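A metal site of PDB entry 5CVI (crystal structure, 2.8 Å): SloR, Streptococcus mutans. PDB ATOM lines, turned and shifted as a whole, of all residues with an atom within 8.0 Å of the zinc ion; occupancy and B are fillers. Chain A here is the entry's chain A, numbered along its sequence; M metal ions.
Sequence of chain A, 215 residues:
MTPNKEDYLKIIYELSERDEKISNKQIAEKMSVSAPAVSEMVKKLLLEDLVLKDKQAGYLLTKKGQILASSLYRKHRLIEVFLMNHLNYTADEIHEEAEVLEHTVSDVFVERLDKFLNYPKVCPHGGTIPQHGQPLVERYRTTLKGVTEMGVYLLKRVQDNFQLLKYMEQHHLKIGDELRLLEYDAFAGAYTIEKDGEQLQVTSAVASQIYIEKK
Lys 10 touches the zinc ion. Within 4 Å of the zinc ion: Asp 7, Lys 10, Glu 99, Glu 102 and His 103.
The zinc ion is bound by OE2 of Glu 99 (1.9 Å), OE2 of Glu 102 (2.0 Å), OD1 of Asp 7 (2.0 Å) and NE2 of His 103 (2.0 Å).
OE1 of Glu 102 lies within hydrogen-bond range of ND1 of His 76 (3.0 Å). The side-chain carboxylate of Glu 99 lies within salt-bridge range of the side-chain amino group of Lys 10 (3.3 Å). OE1 of Glu 102 lies within salt-bridge range of NZ of Lys 10. OD2 of Asp 7 lies close to OD1 of Asn 4, 3.3 Å away. A ring nitrogen (ND1) of His 103 sits close to the side-chain amide nitrogen of Asn 4, at 3.4 Å.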
ATOM      1  N   PRO A   3      26.948   0.895   0.486  1.00  0.00           N
ATOM      2  CA  PRO A   3      26.535   1.706  -0.666  1.00  0.00           C
ATOM      3  C   PRO A   3      25.320   2.566  -0.343  1.00  0.00           C
ATOM      4  O   PRO A   3      24.214   2.031  -0.228  1.00  0.00           O
ATOM      5  CB  PRO A   3      26.164   0.659  -1.719  1.00  0.00           C
ATOM      6  CG  PRO A   3      26.893  -0.569  -1.321  1.00  0.00           C
ATOM      7  CD  PRO A   3      26.929  -0.547   0.181  1.00  0.00           C
ATOM      8  N   ASN A   4      25.512   3.874  -0.207  1.00  0.00           N
ATOM      9  CA  ASN A   4      24.414   4.781   0.120  1.00  0.00           C
ATOM     10  C   ASN A   4      23.424   4.929  -1.039  1.00  0.00           C
ATOM     11  O   ASN A   4      23.611   4.335  -2.105  1.00  0.00           O
ATOM     12  CB  ASN A   4      24.945   6.147   0.545  1.00  0.00           C
ATOM     13  CG  ASN A   4      25.744   6.824  -0.546  1.00  0.00           C
ATOM     14  OD1 ASN A   4      26.345   6.173  -1.402  1.00  0.00           O
ATOM     15  ND2 ASN A   4      25.765   8.161  -0.523  1.00  0.00           N
ATOM     16  N   LYS A   5      22.373   5.705  -0.819  1.00  0.00           N
ATOM     17  CA  LYS A   5      21.324   5.882  -1.826  1.00  0.00           C
ATOM     18  C   LYS A   5      21.854   6.441  -3.138  1.00  0.00           C
ATOM     19  O   LYS A   5      21.377   6.091  -4.208  1.00  0.00           O
ATOM     20  CB  LYS A   5      20.202   6.784  -1.288  1.00  0.00           C
ATOM     21  CG  LYS A   5      20.648   8.185  -0.935  1.00  0.00           C
ATOM     22  CD  LYS A   5      19.476   9.099  -0.624  1.00  0.00           C
ATOM     23  CE  LYS A   5      19.963  10.500  -0.280  1.00  0.00           C
ATOM     24  NZ  LYS A   5      18.852  11.435   0.013  1.00  0.00           N
ATOM     25  N   GLU A   6      22.860   7.315  -3.040  1.00  0.00           N
ATOM     26  CA  GLU A   6      23.428   7.960  -4.218  1.00  0.00           C
ATOM     27  C   GLU A   6      24.061   6.951  -5.166  1.00  0.00           C
ATOM     28  O   GLU A   6      24.141   7.185  -6.377  1.00  0.00           O
ATOM     29  CB  GLU A   6      24.441   9.028  -3.790  1.00  0.00           C
ATOM     30  CG  GLU A   6      23.831  10.142  -2.957  1.00  0.00           C
ATOM     31  CD  GLU A   6      24.847  10.857  -2.091  1.00  0.00           C
ATOM     32  OE1 GLU A   6      25.121  10.368  -0.971  1.00  0.00           O
ATOM     33  OE2 GLU A   6      25.359  11.911  -2.522  1.00  0.00           O
ATOM     34  N   ASP A   7      24.516   5.827  -4.617  1.00  0.00           N
ATOM     35  CA  ASP A   7      25.098   4.765  -5.426  1.00  0.00           C
ATOM     36  C   ASP A   7      24.052   4.120  -6.324  1.00  0.00           C
ATOM     37  O   ASP A   7      24.338   3.728  -7.458  1.00  0.00           O
ATOM     38  CB  ASP A   7      25.752   3.718  -4.537  1.00  0.00           C
ATOM     39  CG  ASP A   7      27.141   4.121  -4.088  1.00  0.00           C
ATOM     40  OD1 ASP A   7      27.780   4.914  -4.810  1.00  0.00           O
ATOM     41  OD2 ASP A   7      27.588   3.647  -3.027  1.00  0.00           O
ATOM     42  N   TYR A   8      22.833   4.020  -5.805  1.00  0.00           N
ATOM     43  CA  TYR A   8      21.715   3.432  -6.535  1.00  0.00           C
ATOM     44  C   TYR A   8      21.349   4.271  -7.762  1.00  0.00           C
ATOM     45  O   TYR A   8      20.892   3.730  -8.770  1.00  0.00           O
ATOM     46  CB  TYR A   8      20.518   3.269  -5.600  1.00  0.00           C
ATOM     47  CG  TYR A   8      20.694   2.161  -4.582  1.00  0.00           C
ATOM     48  CD1 TYR A   8      20.037   0.947  -4.736  1.00  0.00           C
ATOM     49  CD2 TYR A   8      21.538   2.318  -3.491  1.00  0.00           C
ATOM     50  CE1 TYR A   8      20.208  -0.076  -3.820  1.00  0.00           C
ATOM     51  CE2 TYR A   8      21.713   1.299  -2.567  1.00  0.00           C
ATOM     52  CZ  TYR A   8      21.040   0.110  -2.738  1.00  0.00           C
ATOM     53  OH  TYR A   8      21.200  -0.903  -1.822  1.00  0.00           O
ATOM     54  N   LYS A  10      23.481   5.970  -9.703  1.00  0.00           N
ATOM     55  CA  LYS A  10      24.449   5.652 -10.744  1.00  0.00           C
ATOM     56  C   LYS A  10      24.130   4.322 -11.409  1.00  0.00           C
ATOM     57  O   LYS A  10      24.413   4.128 -12.592  1.00  0.00           O
ATOM     58  CB  LYS A  10      25.875   5.638 -10.176  1.00  0.00           C
ATOM     59  CG  LYS A  10      26.342   6.989  -9.648  1.00  0.00           C
ATOM     60  CD  LYS A  10      27.833   7.003  -9.374  1.00  0.00           C
ATOM     61  CE  LYS A  10      28.224   5.951  -8.335  1.00  0.00           C
ATOM     62  NZ  LYS A  10      29.704   5.836  -8.199  1.00  0.00           N
ATOM     63  N   LEU A  72      28.079  13.217  -9.137  1.00  0.00           N
ATOM     64  CA  LEU A  72      28.769  12.030  -8.640  1.00  0.00           C
ATOM     65  C   LEU A  72      29.808  11.521  -9.633  1.00  0.00           C
ATOM     66  O   LEU A  72      30.934  11.216  -9.243  1.00  0.00           O
ATOM     67  CB  LEU A  72      27.777  10.914  -8.301  1.00  0.00           C
ATOM     68  CG  LEU A  72      27.419  10.749  -6.821  1.00  0.00           C
ATOM     69  CD1 LEU A  72      27.627   9.306  -6.378  1.00  0.00           C
ATOM     70  CD2 LEU A  72      28.252  11.701  -5.970  1.00  0.00           C
ATOM     71  N   HIS A  76      33.833  11.297  -9.050  1.00  0.00           N
ATOM     72  CA  HIS A  76      34.441   9.984  -9.250  1.00  0.00           C
ATOM     73  C   HIS A  76      35.543  10.022 -10.294  1.00  0.00           C
ATOM     74  O   HIS A  76      36.636   9.495 -10.070  1.00  0.00           O
ATOM     75  CB  HIS A  76      33.363   8.981  -9.664  1.00  0.00           C
ATOM     76  CG  HIS A  76      33.791   7.552  -9.514  1.00  0.00           C
ATOM     77  ND1 HIS A  76      33.747   6.893  -8.303  1.00  0.00           N
ATOM     78  CD2 HIS A  76      34.246   6.655 -10.416  1.00  0.00           C
ATOM     79  CE1 HIS A  76      34.177   5.651  -8.472  1.00  0.00           C
ATOM     80  NE2 HIS A  76      34.478   5.486  -9.741  1.00  0.00           N
ATOM     81  N   HIS A  95      38.774   1.988  -8.097  1.00  0.00           N
ATOM     82  CA  HIS A  95      37.343   2.118  -7.846  1.00  0.00           C
ATOM     83  C   HIS A  95      36.983   2.353  -6.384  1.00  0.00           C
ATOM     84  O   HIS A  95      36.376   3.375  -6.048  1.00  0.00           O
ATOM     85  CB  HIS A  95      36.543   0.935  -8.386  1.00  0.00           C
ATOM     86  CG  HIS A  95      35.067   1.091  -8.211  1.00  0.00           C
ATOM     87  ND1 HIS A  95      34.349   2.051  -8.887  1.00  0.00           N
ATOM     88  CD2 HIS A  95      34.181   0.430  -7.429  1.00  0.00           C
ATOM     89  CE1 HIS A  95      33.080   1.982  -8.530  1.00  0.00           C
ATOM     90  NE2 HIS A  95      32.949   0.997  -7.651  1.00  0.00           N
ATOM     91  N   ALA A  98      38.205   5.683  -5.154  1.00  0.00           N
ATOM     92  CA  ALA A  98      37.433   6.779  -5.735  1.00  0.00           C
ATOM     93  C   ALA A  98      35.994   6.758  -5.230  1.00  0.00           C
ATOM     94  O   ALA A  98      35.334   7.779  -5.151  1.00  0.00           O
ATOM     95  CB  ALA A  98      37.461   6.702  -7.254  1.00  0.00           C
ATOM     96  N   GLU A  99      35.531   5.564  -4.901  1.00  0.00           N
ATOM     97  CA  GLU A  99      34.183   5.364  -4.400  1.00  0.00           C
ATOM     98  C   GLU A  99      34.010   5.989  -3.024  1.00  0.00           C
ATOM     99  O   GLU A  99      32.999   6.654  -2.768  1.00  0.00           O
ATOM    100  CB  GLU A  99      33.862   3.854  -4.342  1.00  0.00           C
ATOM    101  CG  GLU A  99      32.488   3.526  -3.824  1.00  0.00           C
ATOM    102  CD  GLU A  99      31.401   4.306  -4.539  1.00  0.00           C
ATOM    103  OE1 GLU A  99      31.553   4.542  -5.762  1.00  0.00           O
ATOM    104  OE2 GLU A  99      30.416   4.691  -3.881  1.00  0.00           O
ATOM    105  N   VAL A 100      34.989   5.782  -2.163  1.00  0.00           N
ATOM    106  CA  VAL A 100      34.961   6.353  -0.821  1.00  0.00           C
ATOM    107  C   VAL A 100      35.087   7.877  -0.849  1.00  0.00           C
ATOM    108  O   VAL A 100      34.334   8.586  -0.167  1.00  0.00           O
ATOM    109  CB  VAL A 100      36.072   5.747   0.076  1.00  0.00           C
ATOM    110  CG1 VAL A 100      36.501   6.721   1.149  1.00  0.00           C
ATOM    111  CG2 VAL A 100      35.598   4.438   0.691  1.00  0.00           C
ATOM    112  N   LEU A 101      36.027   8.371  -1.647  1.00  0.00           N
ATOM    113  CA  LEU A 101      36.312   9.795  -1.717  1.00  0.00           C
ATOM    114  C   LEU A 101      35.179  10.647  -2.284  1.00  0.00           C
ATOM    115  O   LEU A 101      34.987  11.795  -1.869  1.00  0.00           O
ATOM    116  CB  LEU A 101      37.600  10.049  -2.523  1.00  0.00           C
ATOM    117  CG  LEU A 101      38.906   9.611  -1.862  1.00  0.00           C
ATOM    118  CD1 LEU A 101      40.090   9.951  -2.745  1.00  0.00           C
ATOM    119  CD2 LEU A 101      39.038  10.283  -0.506  1.00  0.00           C
ATOM    120  N   GLU A 102      34.428  10.099  -3.236  1.00  0.00           N
ATOM    121  CA  GLU A 102      33.341  10.848  -3.873  1.00  0.00           C
ATOM    122  C   GLU A 102      32.229  11.162  -2.854  1.00  0.00           C
ATOM    123  O   GLU A 102      31.429  12.065  -3.075  1.00  0.00           O
ATOM    124  CB  GLU A 102      32.766  10.089  -5.067  1.00  0.00           C
ATOM    125  CG  GLU A 102      31.831   8.941  -4.691  1.00  0.00           C
ATOM    126  CD  GLU A 102      31.183   8.279  -5.896  1.00  0.00           C
ATOM    127  OE1 GLU A 102      31.610   8.551  -7.034  1.00  0.00           O
ATOM    128  OE2 GLU A 102      30.239   7.494  -5.689  1.00  0.00           O
ATOM    129  N   HIS A 103      32.202  10.419  -1.757  1.00  0.00           N
ATOM    130  CA  HIS A 103      31.200  10.633  -0.719  1.00  0.00           C
ATOM    131  C   HIS A 103      31.757  11.394   0.483  1.00  0.00           C
ATOM    132  O   HIS A 103      31.049  11.624   1.460  1.00  0.00           O
ATOM    133  CB  HIS A 103      30.614   9.294  -0.266  1.00  0.00           C
ATOM    134  CG  HIS A 103      29.832   8.597  -1.323  1.00  0.00           C
ATOM    135  ND1 HIS A 103      28.702   9.130  -1.889  1.00  0.00           N
ATOM    136  CD2 HIS A 103      30.023   7.398  -1.921  1.00  0.00           C
ATOM    137  CE1 HIS A 103      28.220   8.291  -2.794  1.00  0.00           C
ATOM    138  NE2 HIS A 103      29.007   7.227  -2.830  1.00  0.00           N
HETATM  139 ZN    ZN M   1      29.321   6.164  -4.525  1.00  0.00          ZN
